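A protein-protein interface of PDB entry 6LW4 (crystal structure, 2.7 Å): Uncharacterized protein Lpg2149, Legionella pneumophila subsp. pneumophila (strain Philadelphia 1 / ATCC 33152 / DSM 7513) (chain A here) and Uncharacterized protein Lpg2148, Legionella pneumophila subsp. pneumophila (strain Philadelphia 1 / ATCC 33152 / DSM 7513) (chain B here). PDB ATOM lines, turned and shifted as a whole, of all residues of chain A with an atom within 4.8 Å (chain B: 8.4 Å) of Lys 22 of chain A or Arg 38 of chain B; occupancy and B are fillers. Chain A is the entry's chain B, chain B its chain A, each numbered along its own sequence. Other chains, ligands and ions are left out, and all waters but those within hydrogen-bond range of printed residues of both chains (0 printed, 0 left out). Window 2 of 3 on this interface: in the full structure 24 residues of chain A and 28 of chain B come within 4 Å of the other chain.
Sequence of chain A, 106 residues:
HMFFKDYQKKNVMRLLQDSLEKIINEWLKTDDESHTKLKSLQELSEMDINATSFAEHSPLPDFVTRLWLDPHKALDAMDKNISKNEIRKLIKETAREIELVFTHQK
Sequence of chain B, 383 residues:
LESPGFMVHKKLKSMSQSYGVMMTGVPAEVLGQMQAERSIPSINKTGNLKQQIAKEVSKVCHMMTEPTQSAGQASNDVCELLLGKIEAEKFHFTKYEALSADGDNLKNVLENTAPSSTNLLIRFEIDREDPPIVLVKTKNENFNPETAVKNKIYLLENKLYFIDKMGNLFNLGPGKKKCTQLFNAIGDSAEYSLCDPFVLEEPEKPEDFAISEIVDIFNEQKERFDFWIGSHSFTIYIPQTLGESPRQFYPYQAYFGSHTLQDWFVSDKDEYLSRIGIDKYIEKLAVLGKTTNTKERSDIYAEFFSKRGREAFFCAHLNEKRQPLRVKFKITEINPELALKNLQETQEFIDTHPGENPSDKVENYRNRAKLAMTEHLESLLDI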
ATOM      1  N   LEU A  15      -5.275  17.178 -12.567  1.00  0.00           N
ATOM      2  CA  LEU A  15      -5.127  15.752 -12.844  1.00  0.00           C
ATOM      3  C   LEU A  15      -5.924  15.353 -14.081  1.00  0.00           C
ATOM      4  O   LEU A  15      -5.449  14.567 -14.915  1.00  0.00           O
ATOM      5  CB  LEU A  15      -5.563  14.942 -11.622  1.00  0.00           C
ATOM      6  CG  LEU A  15      -5.389  13.427 -11.646  1.00  0.00           C
ATOM      7  CD1 LEU A  15      -3.923  13.058 -11.752  1.00  0.00           C
ATOM      8  CD2 LEU A  15      -6.002  12.823 -10.393  1.00  0.00           C
ATOM      9  N   ASP A  18      -3.991  16.557 -17.171  1.00  0.00           N
ATOM     10  CA  ASP A  18      -2.828  15.724 -17.467  1.00  0.00           C
ATOM     11  C   ASP A  18      -3.245  14.386 -18.073  1.00  0.00           C
ATOM     12  O   ASP A  18      -2.610  13.896 -19.021  1.00  0.00           O
ATOM     13  CB  ASP A  18      -1.997  15.510 -16.202  1.00  0.00           C
ATOM     14  CG  ASP A  18      -1.241  16.756 -15.790  1.00  0.00           C
ATOM     15  OD1 ASP A  18      -1.246  17.736 -16.564  1.00  0.00           O
ATOM     16  OD2 ASP A  18      -0.638  16.760 -14.696  1.00  0.00           O
ATOM     17  N   SER A  19      -4.310  13.782 -17.544  1.00  0.00           N
ATOM     18  CA  SER A  19      -4.792  12.529 -18.114  1.00  0.00           C
ATOM     19  C   SER A  19      -5.278  12.725 -19.546  1.00  0.00           C
ATOM     20  O   SER A  19      -5.000  11.895 -20.424  1.00  0.00           O
ATOM     21  CB  SER A  19      -5.896  11.955 -17.231  1.00  0.00           C
ATOM     22  OG  SER A  19      -5.575  12.150 -15.865  1.00  0.00           O
ATOM     23  N   LEU A  20      -6.007  13.815 -19.799  1.00  0.00           N
ATOM     24  CA  LEU A  20      -6.434  14.117 -21.162  1.00  0.00           C
ATOM     25  C   LEU A  20      -5.234  14.300 -22.080  1.00  0.00           C
ATOM     26  O   LEU A  20      -5.235  13.821 -23.220  1.00  0.00           O
ATOM     27  CB  LEU A  20      -7.313  15.367 -21.173  1.00  0.00           C
ATOM     28  CG  LEU A  20      -8.805  15.162 -20.908  1.00  0.00           C
ATOM     29  CD1 LEU A  20      -9.484  16.491 -20.602  1.00  0.00           C
ATOM     30  CD2 LEU A  20      -9.468  14.475 -22.091  1.00  0.00           C
ATOM     31  N   GLU A  21      -4.199  14.992 -21.594  1.00  0.00           N
ATOM     32  CA  GLU A  21      -2.974  15.161 -22.368  1.00  0.00           C
ATOM     33  C   GLU A  21      -2.397  13.814 -22.777  1.00  0.00           C
ATOM     34  O   GLU A  21      -2.136  13.576 -23.960  1.00  0.00           O
ATOM     35  CB  GLU A  21      -1.946  15.960 -21.562  1.00  0.00           C
ATOM     36  CG  GLU A  21      -2.165  17.471 -21.569  1.00  0.00           C
ATOM     37  CD  GLU A  21      -1.159  18.220 -20.702  1.00  0.00           C
ATOM     38  OE1 GLU A  21      -0.029  17.717 -20.515  1.00  0.00           O
ATOM     39  OE2 GLU A  21      -1.503  19.314 -20.206  1.00  0.00           O
ATOM     40  N   LYS A  22      -2.194  12.918 -21.809  1.00  0.00           N
ATOM     41  CA  LYS A  22      -1.592  11.619 -22.115  1.00  0.00           C
ATOM     42  C   LYS A  22      -2.441  10.831 -23.111  1.00  0.00           C
ATOM     43  O   LYS A  22      -1.926  10.294 -24.111  1.00  0.00           O
ATOM     44  CB  LYS A  22      -1.392  10.823 -20.826  1.00  0.00           C
ATOM     45  CG  LYS A  22      -0.702   9.484 -21.016  1.00  0.00           C
ATOM     46  CD  LYS A  22      -0.567   8.737 -19.693  1.00  0.00           C
ATOM     47  CE  LYS A  22      -0.530   7.222 -19.896  1.00  0.00           C
ATOM     48  NZ  LYS A  22      -1.262   6.779 -21.120  1.00  0.00           N
ATOM     49  N   ILE A  23      -3.751  10.758 -22.856  1.00  0.00           N
ATOM     50  CA  ILE A  23      -4.638   9.967 -23.706  1.00  0.00           C
ATOM     51  C   ILE A  23      -4.617  10.491 -25.137  1.00  0.00           C
ATOM     52  O   ILE A  23      -4.415   9.728 -26.091  1.00  0.00           O
ATOM     53  CB  ILE A  23      -6.066   9.952 -23.133  1.00  0.00           C
ATOM     54  CG1 ILE A  23      -6.083   9.238 -21.785  1.00  0.00           C
ATOM     55  CG2 ILE A  23      -7.019   9.263 -24.092  1.00  0.00           C
ATOM     56  CD1 ILE A  23      -5.303   7.951 -21.803  1.00  0.00           C
ATOM     57  N   ILE A  24      -4.812  11.803 -25.306  1.00  0.00           N
ATOM     58  CA  ILE A  24      -4.908  12.360 -26.652  1.00  0.00           C
ATOM     59  C   ILE A  24      -3.549  12.363 -27.344  1.00  0.00           C
ATOM     60  O   ILE A  24      -3.477  12.230 -28.569  1.00  0.00           O
ATOM     61  CB  ILE A  24      -5.538  13.765 -26.600  1.00  0.00           C
ATOM     62  CG1 ILE A  24      -6.966  13.681 -26.059  1.00  0.00           C
ATOM     63  CG2 ILE A  24      -5.536  14.421 -27.970  1.00  0.00           C
ATOM     64  CD1 ILE A  24      -7.619  15.029 -25.871  1.00  0.00           C
ATOM     65  N   ASN A  25      -2.453  12.473 -26.589  1.00  0.00           N
ATOM     66  CA  ASN A  25      -1.127  12.358 -27.190  1.00  0.00           C
ATOM     67  C   ASN A  25      -0.933  10.992 -27.830  1.00  0.00           C
ATOM     68  O   ASN A  25      -0.599  10.889 -29.021  1.00  0.00           O
ATOM     69  CB  ASN A  25      -0.044  12.608 -26.137  1.00  0.00           C
ATOM     70  CG  ASN A  25       0.265  14.078 -25.956  1.00  0.00           C
ATOM     71  OD1 ASN A  25       0.327  14.575 -24.833  1.00  0.00           O
ATOM     72  ND2 ASN A  25       0.452  14.786 -27.066  1.00  0.00           N
ATOM     73  N   GLU A  26      -1.137   9.924 -27.052  1.00  0.00           N
ATOM     74  CA  GLU A  26      -0.903   8.601 -27.620  1.00  0.00           C
ATOM     75  C   GLU A  26      -1.959   8.229 -28.656  1.00  0.00           C
ATOM     76  O   GLU A  26      -1.685   7.428 -29.556  1.00  0.00           O
ATOM     77  CB  GLU A  26      -0.814   7.554 -26.514  1.00  0.00           C
ATOM     78  CG  GLU A  26       0.511   7.622 -25.769  1.00  0.00           C
ATOM     79  CD  GLU A  26       0.479   6.947 -24.416  1.00  0.00           C
ATOM     80  OE1 GLU A  26       1.347   7.270 -23.577  1.00  0.00           O
ATOM     81  OE2 GLU A  26      -0.397   6.083 -24.196  1.00  0.00           O
ATOM     82  N   VAL B  30     -11.637   9.630  -7.327  1.00  0.00           N
ATOM     83  CA  VAL B  30     -11.239  10.453  -8.471  1.00  0.00           C
ATOM     84  C   VAL B  30      -9.924   9.946  -9.051  1.00  0.00           C
ATOM     85  O   VAL B  30      -9.780   9.758 -10.271  1.00  0.00           O
ATOM     86  CB  VAL B  30     -11.124  11.928  -8.045  1.00  0.00           C
ATOM     87  CG1 VAL B  30     -10.484  12.757  -9.142  1.00  0.00           C
ATOM     88  CG2 VAL B  30     -12.481  12.481  -7.664  1.00  0.00           C
ATOM     89  N   LEU B  31      -8.938   9.740  -8.173  1.00  0.00           N
ATOM     90  CA  LEU B  31      -7.633   9.247  -8.594  1.00  0.00           C
ATOM     91  C   LEU B  31      -7.750   7.902  -9.297  1.00  0.00           C
ATOM     92  O   LEU B  31      -7.146   7.692 -10.356  1.00  0.00           O
ATOM     93  CB  LEU B  31      -6.713   9.144  -7.379  1.00  0.00           C
ATOM     94  CG  LEU B  31      -5.258   8.738  -7.608  1.00  0.00           C
ATOM     95  CD1 LEU B  31      -4.554   9.768  -8.473  1.00  0.00           C
ATOM     96  CD2 LEU B  31      -4.549   8.572  -6.277  1.00  0.00           C
ATOM     97  N   GLY B  32      -8.532   6.983  -8.725  1.00  0.00           N
ATOM     98  CA  GLY B  32      -8.688   5.674  -9.335  1.00  0.00           C
ATOM     99  C   GLY B  32      -9.397   5.728 -10.673  1.00  0.00           C
ATOM    100  O   GLY B  32      -9.024   5.019 -11.610  1.00  0.00           O
ATOM    101  N   GLN B  33     -10.407   6.559 -10.783  1.00  0.00           N
ATOM    102  CA  GLN B  33     -11.151   6.683 -12.053  1.00  0.00           C
ATOM    103  C   GLN B  33     -10.278   7.285 -13.147  1.00  0.00           C
ATOM    104  O   GLN B  33     -10.483   6.989 -14.276  1.00  0.00           O
ATOM    105  CB  GLN B  33     -12.405   7.510 -11.836  1.00  0.00           C
ATOM    106  CG  GLN B  33     -13.456   6.794 -11.049  1.00  0.00           C
ATOM    107  CD  GLN B  33     -14.691   7.636 -11.090  1.00  0.00           C
ATOM    108  OE1 GLN B  33     -14.636   8.825 -11.275  1.00  0.00           O
ATOM    109  NE2 GLN B  33     -15.822   7.008 -10.936  1.00  0.00           N
ATOM    110  N   MET B  34      -9.479   8.266 -12.805  1.00  0.00           N
ATOM    111  CA  MET B  34      -8.599   8.883 -13.805  1.00  0.00           C
ATOM    112  C   MET B  34      -7.472   7.930 -14.193  1.00  0.00           C
ATOM    113  O   MET B  34      -7.009   7.988 -15.283  1.00  0.00           O
ATOM    114  CB  MET B  34      -8.141  10.261 -13.344  1.00  0.00           C
ATOM    115  CG  MET B  34      -9.108  11.283 -13.809  1.00  0.00           C
ATOM    116  SD  MET B  34      -8.815  12.878 -13.202  1.00  0.00           S
ATOM    117  CE  MET B  34     -10.468  13.435 -12.880  1.00  0.00           C
ATOM    118  N   GLN B  35      -6.989   7.163 -13.244  1.00  0.00           N
ATOM    119  CA  GLN B  35      -5.953   6.168 -13.521  1.00  0.00           C
ATOM    120  C   GLN B  35      -6.540   5.122 -14.446  1.00  0.00           C
ATOM    121  O   GLN B  35      -5.884   4.697 -15.314  1.00  0.00           O
ATOM    122  CB  GLN B  35      -5.584   5.491 -12.218  1.00  0.00           C
ATOM    123  CG  GLN B  35      -4.145   5.655 -11.790  1.00  0.00           C
ATOM    124  CD  GLN B  35      -3.175   5.995 -12.885  1.00  0.00           C
ATOM    125  OE1 GLN B  35      -2.762   7.133 -13.011  1.00  0.00           O
ATOM    126  NE2 GLN B  35      -2.789   5.012 -13.667  1.00  0.00           N
ATOM    127  N   ALA B  36      -7.757   4.703 -14.196  1.00  0.00           N
ATOM    128  CA  ALA B  36      -8.404   3.729 -15.066  1.00  0.00           C
ATOM    129  C   ALA B  36      -8.533   4.266 -16.482  1.00  0.00           C
ATOM    130  O   ALA B  36      -8.262   3.551 -17.458  1.00  0.00           O
ATOM    131  CB  ALA B  36      -9.779   3.361 -14.505  1.00  0.00           C
ATOM    132  N   GLU B  37      -8.948   5.531 -16.614  1.00  0.00           N
ATOM    133  CA  GLU B  37      -9.113   6.111 -17.942  1.00  0.00           C
ATOM    134  C   GLU B  37      -7.791   6.158 -18.694  1.00  0.00           C
ATOM    135  O   GLU B  37      -7.757   5.953 -19.914  1.00  0.00           O
ATOM    136  CB  GLU B  37      -9.726   7.506 -17.843  1.00  0.00           C
ATOM    137  CG  GLU B  37     -11.184   7.509 -17.428  1.00  0.00           C
ATOM    138  CD  GLU B  37     -12.098   6.861 -18.459  1.00  0.00           C
ATOM    139  OE1 GLU B  37     -13.288   6.654 -18.145  1.00  0.00           O
ATOM    140  OE2 GLU B  37     -11.638   6.568 -19.583  1.00  0.00           O
ATOM    141  N   ARG B  38      -6.690   6.420 -17.991  1.00  0.00           N
ATOM    142  CA  ARG B  38      -5.407   6.487 -18.677  1.00  0.00           C
ATOM    143  C   ARG B  38      -4.726   5.130 -18.816  1.00  0.00           C
ATOM    144  O   ARG B  38      -3.773   5.012 -19.596  1.00  0.00           O
ATOM    145  CB  ARG B  38      -4.463   7.471 -17.977  1.00  0.00           C
ATOM    146  CG  ARG B  38      -4.096   7.124 -16.554  1.00  0.00           C
ATOM    147  CD  ARG B  38      -2.718   7.679 -16.232  1.00  0.00           C
ATOM    148  NE  ARG B  38      -2.701   9.139 -16.245  1.00  0.00           N
ATOM    149  CZ  ARG B  38      -3.026   9.899 -15.205  1.00  0.00           C
ATOM    150  NH1 ARG B  38      -3.390   9.337 -14.061  1.00  0.00           N
ATOM    151  NH2 ARG B  38      -2.980  11.221 -15.305  1.00  0.00           N
ATOM    152  N   SER B  39      -5.190   4.108 -18.098  1.00  0.00           N
ATOM    153  CA  SER B  39      -4.622   2.773 -18.220  1.00  0.00           C
ATOM    154  C   SER B  39      -5.392   1.878 -19.178  1.00  0.00           C
ATOM    155  O   SER B  39      -4.848   0.861 -19.620  1.00  0.00           O
ATOM    156  CB  SER B  39      -4.567   2.091 -16.849  1.00  0.00           C
ATOM    157  OG  SER B  39      -3.517   2.611 -16.052  1.00  0.00           O
ATOM    158  N   ILE B  40      -6.636   2.218 -19.503  1.00  0.00           N
ATOM    159  CA  ILE B  40      -7.463   1.310 -20.300  1.00  0.00           C
ATOM    160  C   ILE B  40      -6.939   1.101 -21.724  1.00  0.00           C
ATOM    161  O   ILE B  40      -7.085  -0.018 -22.239  1.00  0.00           O
ATOM    162  CB  ILE B  40      -8.940   1.754 -20.301  1.00  0.00           C
ATOM    163  CG1 ILE B  40      -9.813   0.677 -20.947  1.00  0.00           C
ATOM    164  CG2 ILE B  40      -9.148   3.097 -20.983  1.00  0.00           C
ATOM    165  CD1 ILE B  40     -11.273   1.009 -20.954  1.00  0.00           C
ATOM    166  N   PRO B  41      -6.317   2.076 -22.408  1.00  0.00           N
ATOM    167  CA  PRO B  41      -5.758   1.748 -23.732  1.00  0.00           C
ATOM    168  C   PRO B  41      -4.666   0.701 -23.667  1.00  0.00           C
ATOM    169  O   PRO B  41      -4.388   0.048 -24.681  1.00  0.00           O
ATOM    170  CB  PRO B  41      -5.214   3.093 -24.238  1.00  0.00           C
ATOM    171  CG  PRO B  41      -5.903   4.118 -23.425  1.00  0.00           C
ATOM    172  CD  PRO B  41      -6.041   3.488 -22.082  1.00  0.00           C
ATOM    173  N   SER B  42      -4.042   0.520 -22.502  1.00  0.00           N
ATOM    174  CA  SER B  42      -3.037  -0.512 -22.288  1.00  0.00           C
ATOM    175  C   SER B  42      -3.640  -1.824 -21.804  1.00  0.00           C
ATOM    176  O   SER B  42      -2.958  -2.600 -21.120  1.00  0.00           O
ATOM    177  CB  SER B  42      -1.985  -0.017 -21.296  1.00  0.00           C
ATOM    178  OG  SER B  42      -2.279  -0.453 -19.980  1.00  0.00           O
ATOM    179  N   ILE B  43      -4.902  -2.090 -22.130  1.00  0.00           N
ATOM    180  CA  ILE B  43      -5.586  -3.307 -21.711  1.00  0.00           C
ATOM    181  C   ILE B  43      -6.161  -3.977 -22.948  1.00  0.00           C
ATOM    182  O   ILE B  43      -6.837  -3.326 -23.752  1.00  0.00           O
ATOM    183  CB  ILE B  43      -6.693  -3.024 -20.681  1.00  0.00           C
ATOM    184  CG1 ILE B  43      -6.091  -2.946 -19.281  1.00  0.00           C
ATOM    185  CG2 ILE B  43      -7.759  -4.101 -20.750  1.00  0.00           C
ATOM    186  CD1 ILE B  43      -7.117  -2.919 -18.196  1.00  0.00           C
ATOM    187  N   GLU B  56      -3.038  -3.678 -13.776  1.00  0.00           N
ATOM    188  CA  GLU B  56      -3.140  -2.228 -13.890  1.00  0.00           C
ATOM    189  C   GLU B  56      -3.393  -1.585 -12.531  1.00  0.00           C
ATOM    190  O   GLU B  56      -2.764  -0.579 -12.176  1.00  0.00           O
ATOM    191  CB  GLU B  56      -4.250  -1.847 -14.864  1.00  0.00           C
ATOM    192  CG  GLU B  56      -3.846  -1.867 -16.348  1.00  0.00           C
ATOM    193  CD  GLU B  56      -2.566  -1.081 -16.629  1.00  0.00           C
ATOM    194  OE1 GLU B  56      -2.322  -0.045 -15.969  1.00  0.00           O
ATOM    195  OE2 GLU B  56      -1.774  -1.530 -17.483  1.00  0.00           O
ATOM    196  N   VAL B  60      -0.757   1.092  -9.018  1.00  0.00           N
ATOM    197  CA  VAL B  60      -0.931   2.385  -8.355  1.00  0.00           C
ATOM    198  C   VAL B  60      -0.836   2.290  -6.838  1.00  0.00           C
ATOM    199  O   VAL B  60      -1.105   3.283  -6.147  1.00  0.00           O
ATOM    200  CB  VAL B  60      -2.246   3.080  -8.768  1.00  0.00           C
ATOM    201  CG1 VAL B  60      -2.433   3.032 -10.272  1.00  0.00           C
ATOM    202  CG2 VAL B  60      -3.457   2.471  -8.015  1.00  0.00           C
ATOM    203  N   MET B  63       1.977   4.199  -8.362  1.00  0.00           N
ATOM    204  CA  MET B  63       1.643   5.517  -8.897  1.00  0.00           C
ATOM    205  C   MET B  63       1.312   6.534  -7.809  1.00  0.00           C
ATOM    206  O   MET B  63       1.221   7.729  -8.113  1.00  0.00           O
ATOM    207  CB  MET B  63       0.463   5.426  -9.868  1.00  0.00           C
ATOM    208  CG  MET B  63       0.279   6.643 -10.809  1.00  0.00           C
ATOM    209  SD  MET B  63       0.812   6.367 -12.522  1.00  0.00           S
ATOM    210  CE  MET B  63       0.539   7.981 -13.252  1.00  0.00           C
ATOM    211  N   THR B  68       5.482  10.750 -10.272  1.00  0.00           N
ATOM    212  CA  THR B  68       4.598  11.230 -11.327  1.00  0.00           C
ATOM    213  C   THR B  68       4.120  12.657 -11.085  1.00  0.00           C
ATOM    214  O   THR B  68       3.132  13.087 -11.690  1.00  0.00           O
ATOM    215  CB  THR B  68       3.392  10.303 -11.472  1.00  0.00           C
ATOM    216  OG1 THR B  68       2.939   9.907 -10.170  1.00  0.00           O
ATOM    217  CG2 THR B  68       3.767   9.070 -12.270  1.00  0.00           C
ATOM    218  N   MET B 373     -10.511   2.286  -9.172  1.00  0.00           N
ATOM    219  CA  MET B 373      -9.884   1.987 -10.456  1.00  0.00           C
ATOM    220  C   MET B 373     -10.395   0.666 -11.022  1.00  0.00           C
ATOM    221  O   MET B 373     -10.733   0.571 -12.210  1.00  0.00           O
ATOM    222  CB  MET B 373      -8.363   1.954 -10.288  1.00  0.00           C
ATOM    223  CG  MET B 373      -7.577   1.923 -11.591  1.00  0.00           C
ATOM    224  SD  MET B 373      -5.792   1.852 -11.306  1.00  0.00           S
ATOM    225  CE  MET B 373      -5.187   1.625 -12.978  1.00  0.00           C
ATOM    226  N   HIS B 376     -14.049   1.023 -12.121  1.00  0.00           N
ATOM    227  CA  HIS B 376     -14.148   1.833 -13.331  1.00  0.00           C
ATOM    228  C   HIS B 376     -13.689   1.048 -14.556  1.00  0.00           C
ATOM    229  O   HIS B 376     -14.280   1.167 -15.639  1.00  0.00           O
ATOM    230  CB  HIS B 376     -13.333   3.114 -13.166  1.00  0.00           C
ATOM    231  CG  HIS B 376     -13.692   4.188 -14.144  1.00  0.00           C
ATOM    232  ND1 HIS B 376     -14.877   4.889 -14.079  1.00  0.00           N
ATOM    233  CD2 HIS B 376     -13.017   4.688 -15.205  1.00  0.00           C
ATOM    234  CE1 HIS B 376     -14.917   5.773 -15.061  1.00  0.00           C
ATOM    235  NE2 HIS B 376     -13.801   5.671 -15.759  1.00  0.00           N
ATOM    236  N   LEU B 377     -12.650   0.223 -14.404  1.00  0.00           N
ATOM    237  CA  LEU B 377     -12.213  -0.606 -15.522  1.00  0.00           C
ATOM    238  C   LEU B 377     -13.259  -1.659 -15.869  1.00  0.00           C
ATOM    239  O   LEU B 377     -13.530  -1.910 -17.049  1.00  0.00           O
ATOM    240  CB  LEU B 377     -10.870  -1.259 -15.199  1.00  0.00           C
ATOM    241  CG  LEU B 377      -9.669  -0.309 -15.226  1.00  0.00           C
ATOM    242  CD1 LEU B 377      -8.500  -0.888 -14.448  1.00  0.00           C
ATOM    243  CD2 LEU B 377      -9.261   0.005 -16.661  1.00  0.00           C
ATOM    244  N   LEU B 380     -15.913  -0.010 -17.795  1.00  0.00           N
ATOM    245  CA  LEU B 380     -15.531   0.293 -19.167  1.00  0.00           C
ATOM    246  C   LEU B 380     -15.271  -0.952 -20.008  1.00  0.00           C
ATOM    247  O   LEU B 380     -15.084  -0.824 -21.223  1.00  0.00           O
ATOM    248  CB  LEU B 380     -14.288   1.185 -19.173  1.00  0.00           C
ATOM    249  CG  LEU B 380     -14.442   2.592 -18.593  1.00  0.00           C
ATOM    250  CD1 LEU B 380     -13.082   3.261 -18.481  1.00  0.00           C
ATOM    251  CD2 LEU B 380     -15.394   3.425 -19.442  1.00  0.00           C
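The guanidinium group (NH2) of Arg 38 of chain B sits at hydrogen-bond distance from the side-chain hydroxyl (OG) of Ser 19 of chain A, 2.8 Å away.
O of Arg 38 of chain B is in hydrogen-bond range of NZ of Lys 22 of chain A (3.4 Å).
OE1 of Gln 35 of chain B lies within hydrogen-bond range of NH1 of Arg 38 of chain B (2.5 Å).
The side-chain carboxylate (OE1) of Glu 37 of chain B lies within hydrogen-bond range of a ring nitrogen (NE2) of His 376 of chain B, at 2.6 Å.
The backbone carbonyl oxygen of Leu 15 of chain A sits at hydrogen-bond distance from the side-chain hydroxyl of Ser 19 of chain A (2.6 Å).
The side-chain amino group (NZ) of Lys 22 of chain A is in salt-bridge range of the side-chain carboxylate (OE2) of Glu 26 of chain A (3.3 Å).
Among the printed residues, pairs that only touch across the chains: Leu 15 of chain A with Leu 31 of chain B (3.9 Å), Leu 15 of chain A with Met 34 of chain B (3.8 Å), Ile 23 of chain A with Glu 37 of chain B (3.7 Å) and Ile 23 of chain A with Arg 38 of chain B (3.5 Å).
Of chain B, only Arg 38 (2.8 Å) comes within 4 Å of Ser 19 of chain A.
Lys 22 of chain A touches just one residue of chain B: Arg 38.
Of the printed residues of chain B, Ile 23 of chain A touches Glu 37 and Arg 38.
Printed residues of chain A within 4 Å of Leu 31 of chain B: Leu 15 (3.9 Å).
Printed residues of chain A within 4 Å of Met 34 of chain B: Leu 15.
Printed residues of chain A within 4 Å of Glu 37 of chain B: Ile 23.
Of chain A, only Ser 19, Lys 22 and Ile 23 come within 4 Å of Arg 38 of chain B.
Ser 42 of chain B touches none of the printed residues of chain A.
The nearest printed residue of chain B that does not touch Ile 23 of chain A is Pro 41 of chain B (4.2 Å).
Of the 10 printed residues of chain A, 4 touch a printed residue of chain B.
Hydrophobic or aromatic side chains of chain A within 4 Å of the printed part of chain B: Leu 15 and Ile 23.
Of the 22 printed residues of chain B, 4 touch a printed residue of chain A.
Among the printed residues, 6 pairs touch across the chains.
Among the printed residues, no Asp or Glu carboxylate lies within 4 Å of a Lys or Arg side-chain nitrogen of the other chain.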
